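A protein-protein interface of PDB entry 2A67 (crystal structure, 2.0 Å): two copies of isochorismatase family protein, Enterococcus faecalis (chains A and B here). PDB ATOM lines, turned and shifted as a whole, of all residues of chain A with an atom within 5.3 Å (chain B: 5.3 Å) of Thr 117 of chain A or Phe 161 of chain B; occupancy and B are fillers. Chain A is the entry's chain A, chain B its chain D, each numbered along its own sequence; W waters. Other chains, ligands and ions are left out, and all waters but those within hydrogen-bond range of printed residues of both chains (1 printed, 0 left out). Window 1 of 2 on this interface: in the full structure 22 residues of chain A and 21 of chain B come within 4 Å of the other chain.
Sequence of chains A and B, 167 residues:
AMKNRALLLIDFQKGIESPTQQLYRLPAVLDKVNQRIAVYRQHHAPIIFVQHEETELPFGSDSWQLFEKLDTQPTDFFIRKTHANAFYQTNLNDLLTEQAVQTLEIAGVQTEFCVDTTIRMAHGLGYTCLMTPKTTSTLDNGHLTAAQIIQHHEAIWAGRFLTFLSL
The backbone carbonyl oxygen (O) of Glu 112 of chain A sits at hydrogen-bond distance from the guanidinium group (NH1) of Arg 120 of chain B, at 3.0 Å.
The side-chain carboxylate (OD1) of Asp 116 of chain A lies within salt-bridge range of the guanidinium group (NE) of Arg 120 of chain B (3.1 Å).
OG1 of Thr 117 of chain A is in hydrogen-bond range of NH1 of Arg 120 of chain B (2.9 Å).
The side-chain sulfur (SD) of Met 121 of chain A lies close to the side-chain amide nitrogen (ND2) of Asn 85 of chain A (3.5 Å).
The side-chain hydroxyl (OG1) of Thr 117 of chain A lies within hydrogen-bond range of the backbone carbonyl oxygen (O) of Phe 113 of chain A, at 2.5 Å.
The side-chain carboxylate of Asp 116 of chain A is in salt-bridge range of the guanidinium group of Arg 120 of chain A, 2.6 Å away.
The backbone carbonyl oxygen of Ile 156 of chain B sits close to the guanidinium group of Arg 160 of chain B (3.2 Å).
Among the printed residues, merely in contact across the chains: His 83 of chain A with His 123 of chain B (3.2 Å), His 83 of chain A with Arg 160 of chain B (2.8 Å), His 83 of chain A with Phe 161 of chain B (3.3 Å), Glu 112 of chain A with Ile 156 of chain B (3.8 Å), Phe 113 of chain A with Arg 120 of chain B (3.5 Å), Phe 113 of chain A with Ile 156 of chain B (3.8 Å), Phe 113 of chain A with Arg 160 of chain B (3.5 Å), Thr 117 of chain A with Phe 161 of chain B (3.3 Å) and Met 121 of chain A with Arg 120 of chain B (3.2 Å).
Printed residues of chain B within 4 Å of Phe 113 of chain A: Arg 120 (3.5 Å), Ile 156 (3.8 Å) and Arg 160 (3.5 Å).
Thr 117 of chain A touches two residues of chain B.
Ile 119 of chain A touches none of the printed residues of chain B.
Printed residues of chain B within 4 Å of Met 121 of chain A: Arg 120 (3.2 Å).
Of the printed residues of chain A, His 123 of chain B touches His 83 (3.2 Å).
Printed residues of chain A within 4 Å of Arg 160 of chain B: His 83 (2.8 Å) and Phe 113 (3.5 Å).
Of the printed residues of chain A, Phe 161 of chain B touches His 83 and Thr 117.
The nearest residue of chain A that does not touch Phe 161 of chain B is Ala 84 of chain A (4.4 Å).
Of the 14 printed residues of chain A, 6 touch a printed residue of chain B.
Hydrophobic or aromatic side chains of chain A within 4 Å of the printed part of chain B: His 83, Phe 113 and Met 121.
Along chain A the printed residues that touch a printed residue of chain B span positions 83 to 121.
Among the printed residues, Asp or Glu carboxylates within 4 Å of a Lys or Arg side-chain nitrogen of the other chain: Asp 116 of chain A with Arg 120 of chain B.
Positions printed for both chains: 119 and 120.
Water W1 lies within hydrogen-bond range of ND2 of Asn 85 of chain A, ND1 of His 123 of chain B and O of Arg 120 of chain B.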
ATOM      1  N   HIS A  83     -18.993   3.899  14.187  1.00  0.00           N
ATOM      2  CA  HIS A  83     -18.175   2.727  14.562  1.00  0.00           C
ATOM      3  C   HIS A  83     -18.722   1.500  13.831  1.00  0.00           C
ATOM      4  O   HIS A  83     -19.855   1.581  13.325  1.00  0.00           O
ATOM      5  CB  HIS A  83     -18.181   2.488  16.091  1.00  0.00           C
ATOM      6  CG  HIS A  83     -17.401   1.265  16.510  1.00  0.00           C
ATOM      7  ND1 HIS A  83     -16.053   1.307  16.852  1.00  0.00           N
ATOM      8  CD2 HIS A  83     -17.768  -0.043  16.594  1.00  0.00           C
ATOM      9  CE1 HIS A  83     -15.634   0.083  17.130  1.00  0.00           C
ATOM     10  NE2 HIS A  83     -16.657  -0.747  16.993  1.00  0.00           N
ATOM     11  N   ALA A  84     -17.944   0.403  13.737  1.00  0.00           N
ATOM     12  CA  ALA A  84     -18.480  -0.873  13.105  1.00  0.00           C
ATOM     13  C   ALA A  84     -19.826  -1.277  13.714  1.00  0.00           C
ATOM     14  O   ALA A  84     -20.780  -1.740  13.015  1.00  0.00           O
ATOM     15  CB  ALA A  84     -17.463  -1.987  13.282  1.00  0.00           C
ATOM     16  N   ASN A  85     -19.960  -1.112  15.024  1.00  0.00           N
ATOM     17  CA  ASN A  85     -21.223  -1.485  15.700  1.00  0.00           C
ATOM     18  C   ASN A  85     -22.378  -0.477  15.402  1.00  0.00           C
ATOM     19  O   ASN A  85     -22.318   0.685  15.828  1.00  0.00           O
ATOM     20  CB  ASN A  85     -20.911  -1.571  17.198  1.00  0.00           C
ATOM     21  CG  ASN A  85     -22.060  -2.135  18.021  1.00  0.00           C
ATOM     22  OD1 ASN A  85     -23.226  -2.154  17.589  1.00  0.00           O
ATOM     23  ND2 ASN A  85     -21.729  -2.566  19.236  1.00  0.00           N
ATOM     24  N   GLU A 112     -17.063  -8.730   7.744  1.00  0.00           N
ATOM     25  CA  GLU A 112     -16.346  -9.053   8.965  1.00  0.00           C
ATOM     26  C   GLU A 112     -16.279  -7.859   9.950  1.00  0.00           C
ATOM     27  O   GLU A 112     -15.851  -8.006  11.097  1.00  0.00           O
ATOM     28  CB  GLU A 112     -14.922  -9.544   8.645  1.00  0.00           C
ATOM     29  CG  GLU A 112     -13.919  -8.454   8.193  1.00  0.00           C
ATOM     30  CD  GLU A 112     -13.886  -8.284   6.684  1.00  0.00           C
ATOM     31  OE1 GLU A 112     -14.958  -8.109   6.050  1.00  0.00           O
ATOM     32  OE2 GLU A 112     -12.781  -8.352   6.135  1.00  0.00           O
ATOM     33  N   PHE A 113     -16.643  -6.670   9.470  1.00  0.00           N
ATOM     34  CA  PHE A 113     -16.577  -5.461  10.304  1.00  0.00           C
ATOM     35  C   PHE A 113     -17.990  -5.103  10.763  1.00  0.00           C
ATOM     36  O   PHE A 113     -18.429  -5.618  11.774  1.00  0.00           O
ATOM     37  CB  PHE A 113     -15.900  -4.341   9.516  1.00  0.00           C
ATOM     38  CG  PHE A 113     -14.446  -4.648   9.184  1.00  0.00           C
ATOM     39  CD1 PHE A 113     -13.514  -4.869  10.219  1.00  0.00           C
ATOM     40  CD2 PHE A 113     -14.031  -4.737   7.900  1.00  0.00           C
ATOM     41  CE1 PHE A 113     -12.164  -5.156   9.949  1.00  0.00           C
ATOM     42  CE2 PHE A 113     -12.685  -4.998   7.608  1.00  0.00           C
ATOM     43  CZ  PHE A 113     -11.747  -5.209   8.643  1.00  0.00           C
ATOM     44  N   CYS A 114     -18.677  -4.215  10.061  1.00  0.00           N
ATOM     45  CA  CYS A 114     -19.903  -3.608  10.546  1.00  0.00           C
ATOM     46  C   CYS A 114     -21.008  -4.666  10.629  1.00  0.00           C
ATOM     47  O   CYS A 114     -21.826  -4.622  11.527  1.00  0.00           O
ATOM     48  CB  CYS A 114     -20.369  -2.503   9.561  1.00  0.00           C
ATOM     49  SG  CYS A 114     -19.021  -1.101   9.333  1.00  0.00           S
ATOM     50  N   VAL A 115     -21.049  -5.581   9.659  1.00  0.00           N
ATOM     51  CA  VAL A 115     -22.153  -6.567   9.626  1.00  0.00           C
ATOM     52  C   VAL A 115     -21.969  -7.576  10.767  1.00  0.00           C
ATOM     53  O   VAL A 115     -22.875  -7.756  11.574  1.00  0.00           O
ATOM     54  CB  VAL A 115     -22.188  -7.268   8.252  1.00  0.00           C
ATOM     55  CG1 VAL A 115     -23.387  -8.285   8.167  1.00  0.00           C
ATOM     56  CG2 VAL A 115     -22.305  -6.210   7.147  1.00  0.00           C
ATOM     57  N   ASP A 116     -20.792  -8.214  10.855  1.00  0.00           N
ATOM     58  CA  ASP A 116     -20.528  -9.127  11.972  1.00  0.00           C
ATOM     59  C   ASP A 116     -20.811  -8.437  13.329  1.00  0.00           C
ATOM     60  O   ASP A 116     -21.521  -8.950  14.192  1.00  0.00           O
ATOM     61  CB  ASP A 116     -19.083  -9.621  11.909  1.00  0.00           C
ATOM     62  CG  ASP A 116     -18.762 -10.659  12.973  1.00  0.00           C
ATOM     63  OD1 ASP A 116     -18.648 -10.318  14.205  1.00  0.00           O
ATOM     64  OD2 ASP A 116     -18.591 -11.829  12.556  1.00  0.00           O
ATOM     65  N   THR A 117     -20.268  -7.241  13.515  1.00  0.00           N
ATOM     66  CA  THR A 117     -20.439  -6.572  14.829  1.00  0.00           C
ATOM     67  C   THR A 117     -21.910  -6.335  15.163  1.00  0.00           C
ATOM     68  O   THR A 117     -22.326  -6.554  16.278  1.00  0.00           O
ATOM     69  CB  THR A 117     -19.680  -5.224  14.830  1.00  0.00           C
ATOM     70  OG1 THR A 117     -18.373  -5.489  14.302  1.00  0.00           O
ATOM     71  CG2 THR A 117     -19.587  -4.647  16.275  1.00  0.00           C
ATOM     72  N   THR A 118     -22.659  -5.836  14.195  1.00  0.00           N
ATOM     73  CA  THR A 118     -24.041  -5.433  14.425  1.00  0.00           C
ATOM     74  C   THR A 118     -24.925  -6.689  14.683  1.00  0.00           C
ATOM     75  O   THR A 118     -25.819  -6.682  15.514  1.00  0.00           O
ATOM     76  CB  THR A 118     -24.549  -4.597  13.236  1.00  0.00           C
ATOM     77  OG1 THR A 118     -23.674  -3.427  13.081  1.00  0.00           O
ATOM     78  CG2 THR A 118     -26.028  -4.179  13.440  1.00  0.00           C
ATOM     79  N   ILE A 119     -24.591  -7.769  14.011  1.00  0.00           N
ATOM     80  CA  ILE A 119     -25.239  -9.070  14.281  1.00  0.00           C
ATOM     81  C   ILE A 119     -24.976  -9.537  15.695  1.00  0.00           C
ATOM     82  O   ILE A 119     -25.915  -9.944  16.403  1.00  0.00           O
ATOM     83  CB  ILE A 119     -24.739 -10.108  13.248  1.00  0.00           C
ATOM     84  CG1 ILE A 119     -25.333  -9.788  11.869  1.00  0.00           C
ATOM     85  CG2 ILE A 119     -25.120 -11.548  13.668  1.00  0.00           C
ATOM     86  CD1 ILE A 119     -24.715 -10.698  10.766  1.00  0.00           C
ATOM     87  N   ARG A 120     -23.702  -9.534  16.131  1.00  0.00           N
ATOM     88  CA  ARG A 120     -23.395 -10.073  17.472  1.00  0.00           C
ATOM     89  C   ARG A 120     -23.981  -9.187  18.540  1.00  0.00           C
ATOM     90  O   ARG A 120     -24.426  -9.691  19.603  1.00  0.00           O
ATOM     91  CB  ARG A 120     -21.860 -10.270  17.709  1.00  0.00           C
ATOM     92  CG  ARG A 120     -21.158 -11.136  16.614  1.00  0.00           C
ATOM     93  CD  ARG A 120     -19.829 -11.712  17.077  1.00  0.00           C
ATOM     94  NE  ARG A 120     -19.014 -12.234  15.982  1.00  0.00           N
ATOM     95  CZ  ARG A 120     -18.262 -13.342  15.999  1.00  0.00           C
ATOM     96  NH1 ARG A 120     -18.170 -14.146  17.055  1.00  0.00           N
ATOM     97  NH2 ARG A 120     -17.570 -13.644  14.912  1.00  0.00           N
ATOM     98  N   MET A 121     -23.951  -7.857  18.290  1.00  0.00           N
ATOM     99  CA  MET A 121     -24.617  -6.920  19.175  1.00  0.00           C
ATOM    100  C   MET A 121     -26.151  -7.125  19.243  1.00  0.00           C
ATOM    101  O   MET A 121     -26.729  -7.117  20.327  1.00  0.00           O
ATOM    102  CB  MET A 121     -24.268  -5.443  18.807  1.00  0.00           C
ATOM    103  CG  MET A 121     -24.704  -4.418  19.849  1.00  0.00           C
ATOM    104  SD  MET A 121     -23.594  -4.513  21.477  1.00  0.00           S
ATOM    105  CE  MET A 121     -22.095  -5.140  20.709  1.00  0.00           C
ATOM    106  N   ALA A 122     -26.781  -7.191  18.087  1.00  0.00           N
ATOM    107  CA  ALA A 122     -28.250  -7.310  18.024  1.00  0.00           C
ATOM    108  C   ALA A 122     -28.641  -8.594  18.717  1.00  0.00           C
ATOM    109  O   ALA A 122     -29.517  -8.585  19.554  1.00  0.00           O
ATOM    110  CB  ALA A 122     -28.688  -7.314  16.636  1.00  0.00           C
ATOM    111  N   ILE B 119     -15.678  -9.484  23.108  1.00  0.00           N
ATOM    112  CA  ILE B 119     -14.892  -8.242  22.785  1.00  0.00           C
ATOM    113  C   ILE B 119     -15.816  -7.207  22.110  1.00  0.00           C
ATOM    114  O   ILE B 119     -15.930  -6.094  22.591  1.00  0.00           O
ATOM    115  CB  ILE B 119     -13.700  -8.566  21.886  1.00  0.00           C
ATOM    116  CG1 ILE B 119     -12.611  -9.277  22.717  1.00  0.00           C
ATOM    117  CG2 ILE B 119     -13.115  -7.254  21.211  1.00  0.00           C
ATOM    118  CD1 ILE B 119     -11.524  -9.885  21.797  1.00  0.00           C
ATOM    119  N   ARG B 120     -16.541  -7.623  21.071  1.00  0.00           N
ATOM    120  CA  ARG B 120     -17.519  -6.755  20.365  1.00  0.00           C
ATOM    121  C   ARG B 120     -18.621  -6.313  21.292  1.00  0.00           C
ATOM    122  O   ARG B 120     -18.976  -5.132  21.297  1.00  0.00           O
ATOM    123  CB  ARG B 120     -18.102  -7.441  19.118  1.00  0.00           C
ATOM    124  CG  ARG B 120     -16.974  -7.865  18.160  1.00  0.00           C
ATOM    125  CD  ARG B 120     -17.433  -7.956  16.735  1.00  0.00           C
ATOM    126  NE  ARG B 120     -16.559  -8.898  15.996  1.00  0.00           N
ATOM    127  CZ  ARG B 120     -16.204  -8.766  14.717  1.00  0.00           C
ATOM    128  NH1 ARG B 120     -16.621  -7.722  13.975  1.00  0.00           N
ATOM    129  NH2 ARG B 120     -15.424  -9.697  14.160  1.00  0.00           N
ATOM    130  N   HIS B 123     -17.049  -3.887  24.081  1.00  0.00           N
ATOM    131  CA  HIS B 123     -16.776  -2.550  23.487  1.00  0.00           C
ATOM    132  C   HIS B 123     -18.132  -1.817  23.323  1.00  0.00           C
ATOM    133  O   HIS B 123     -18.328  -0.602  23.619  1.00  0.00           O
ATOM    134  CB  HIS B 123     -16.129  -2.711  22.104  1.00  0.00           C
ATOM    135  CG  HIS B 123     -16.084  -1.412  21.346  1.00  0.00           C
ATOM    136  ND1 HIS B 123     -17.148  -0.929  20.598  1.00  0.00           N
ATOM    137  CD2 HIS B 123     -15.142  -0.438  21.343  1.00  0.00           C
ATOM    138  CE1 HIS B 123     -16.823   0.265  20.110  1.00  0.00           C
ATOM    139  NE2 HIS B 123     -15.621   0.588  20.561  1.00  0.00           N
ATOM    140  N   CYS B 129     -11.421  -1.942  26.229  1.00  0.00           N
ATOM    141  CA  CYS B 129     -10.901  -3.312  26.120  1.00  0.00           C
ATOM    142  C   CYS B 129      -9.428  -3.294  25.771  1.00  0.00           C
ATOM    143  O   CYS B 129      -8.980  -2.410  25.004  1.00  0.00           O
ATOM    144  CB  CYS B 129     -11.693  -4.115  25.084  1.00  0.00           C
ATOM    145  SG  CYS B 129     -13.424  -4.217  25.618  1.00  0.00           S
ATOM    146  N   ILE B 156      -8.833  -7.617  13.131  1.00  0.00           N
ATOM    147  CA  ILE B 156     -10.090  -6.854  13.257  1.00  0.00           C
ATOM    148  C   ILE B 156     -10.178  -6.121  14.621  1.00  0.00           C
ATOM    149  O   ILE B 156     -10.610  -4.980  14.697  1.00  0.00           O
ATOM    150  CB  ILE B 156     -11.313  -7.773  13.149  1.00  0.00           C
ATOM    151  CG1 ILE B 156     -11.397  -8.431  11.747  1.00  0.00           C
ATOM    152  CG2 ILE B 156     -12.614  -6.981  13.463  1.00  0.00           C
ATOM    153  CD1 ILE B 156     -12.459  -9.545  11.716  1.00  0.00           C
ATOM    154  N   TRP B 157      -9.800  -6.790  15.699  1.00  0.00           N
ATOM    155  CA  TRP B 157      -9.938  -6.211  17.021  1.00  0.00           C
ATOM    156  C   TRP B 157      -8.972  -5.018  17.256  1.00  0.00           C
ATOM    157  O   TRP B 157      -9.357  -4.054  17.899  1.00  0.00           O
ATOM    158  CB  TRP B 157      -9.645  -7.245  18.089  1.00  0.00           C
ATOM    159  CG  TRP B 157     -10.489  -8.543  17.963  1.00  0.00           C
ATOM    160  CD1 TRP B 157     -11.760  -8.710  17.404  1.00  0.00           C
ATOM    161  CD2 TRP B 157     -10.115  -9.795  18.495  1.00  0.00           C
ATOM    162  NE1 TRP B 157     -12.145 -10.053  17.520  1.00  0.00           N
ATOM    163  CE2 TRP B 157     -11.178 -10.719  18.228  1.00  0.00           C
ATOM    164  CE3 TRP B 157      -8.968 -10.242  19.176  1.00  0.00           C
ATOM    165  CZ2 TRP B 157     -11.107 -12.078  18.577  1.00  0.00           C
ATOM    166  CZ3 TRP B 157      -8.893 -11.595  19.556  1.00  0.00           C
ATOM    167  CH2 TRP B 157     -10.006 -12.519  19.246  1.00  0.00           C
ATOM    168  N   ALA B 158      -7.768  -5.104  16.732  1.00  0.00           N
ATOM    169  CA  ALA B 158      -6.720  -4.086  17.023  1.00  0.00           C
ATOM    170  C   ALA B 158      -7.221  -2.718  16.647  1.00  0.00           C
ATOM    171  O   ALA B 158      -7.585  -2.476  15.485  1.00  0.00           O
ATOM    172  CB  ALA B 158      -5.450  -4.408  16.270  1.00  0.00           C
ATOM    173  N   GLY B 159      -7.306  -1.832  17.635  1.00  0.00           N
ATOM    174  CA  GLY B 159      -7.651  -0.446  17.336  1.00  0.00           C
ATOM    175  C   GLY B 159      -9.152  -0.213  17.280  1.00  0.00           C
ATOM    176  O   GLY B 159      -9.679   0.736  17.878  1.00  0.00           O
ATOM    177  N   ARG B 160      -9.916  -1.104  16.642  1.00  0.00           N
ATOM    178  CA  ARG B 160     -11.339  -0.797  16.599  1.00  0.00           C
ATOM    179  C   ARG B 160     -12.139  -1.233  17.804  1.00  0.00           C
ATOM    180  O   ARG B 160     -13.077  -0.522  18.214  1.00  0.00           O
ATOM    181  CB  ARG B 160     -11.940  -1.179  15.264  1.00  0.00           C
ATOM    182  CG  ARG B 160     -12.059  -2.566  15.059  1.00  0.00           C
ATOM    183  CD  ARG B 160     -13.150  -2.853  14.048  1.00  0.00           C
ATOM    184  NE  ARG B 160     -12.947  -2.209  12.752  1.00  0.00           N
ATOM    185  CZ  ARG B 160     -11.886  -2.287  11.957  1.00  0.00           C
ATOM    186  NH1 ARG B 160     -10.776  -2.971  12.272  1.00  0.00           N
ATOM    187  NH2 ARG B 160     -11.959  -1.644  10.800  1.00  0.00           N
ATOM    188  N   PHE B 161     -11.740  -2.321  18.448  1.00  0.00           N
ATOM    189  CA  PHE B 161     -12.445  -2.724  19.651  1.00  0.00           C
ATOM    190  C   PHE B 161     -11.577  -2.666  20.904  1.00  0.00           C
ATOM    191  O   PHE B 161     -12.119  -2.609  22.023  1.00  0.00           O
ATOM    192  CB  PHE B 161     -13.010  -4.174  19.561  1.00  0.00           C
ATOM    193  CG  PHE B 161     -14.029  -4.363  18.444  1.00  0.00           C
ATOM    194  CD1 PHE B 161     -15.303  -3.835  18.542  1.00  0.00           C
ATOM    195  CD2 PHE B 161     -13.706  -5.090  17.318  1.00  0.00           C
ATOM    196  CE1 PHE B 161     -16.227  -3.990  17.485  1.00  0.00           C
ATOM    197  CE2 PHE B 161     -14.625  -5.258  16.261  1.00  0.00           C
ATOM    198  CZ  PHE B 161     -15.872  -4.678  16.339  1.00  0.00           C
ATOM    199  N   LEU B 162     -10.263  -2.815  20.725  1.00  0.00           N
ATOM    200  CA  LEU B 162      -9.352  -2.970  21.881  1.00  0.00           C
ATOM    201  C   LEU B 162      -7.947  -2.472  21.507  1.00  0.00           C
ATOM    202  O   LEU B 162      -7.661  -2.187  20.352  1.00  0.00           O
ATOM    203  CB  LEU B 162      -9.338  -4.433  22.421  1.00  0.00           C
ATOM    204  CG  LEU B 162      -8.955  -5.603  21.468  1.00  0.00           C
ATOM    205  CD1 LEU B 162      -7.439  -5.550  21.123  1.00  0.00           C
ATOM    206  CD2 LEU B 162      -9.273  -6.930  22.159  1.00  0.00           C
ATOM    207  N   THR B 163      -7.098  -2.320  22.512  1.00  0.00           N
ATOM    208  CA  THR B 163      -5.704  -2.014  22.286  1.00  0.00           C
ATOM    209  C   THR B 163      -4.907  -3.228  22.674  1.00  0.00           C
ATOM    210  O   THR B 163      -5.069  -3.713  23.792  1.00  0.00           O
ATOM    211  CB  THR B 163      -5.253  -0.841  23.240  1.00  0.00           C
ATOM    212  OG1 THR B 163      -6.111   0.295  23.071  1.00  0.00           O
ATOM    213  CG2 THR B 163      -3.769  -0.419  22.949  1.00  0.00           C
HETATM  214  O   HOH W   1     -18.944  -2.820  19.473  1.00  0.00           O
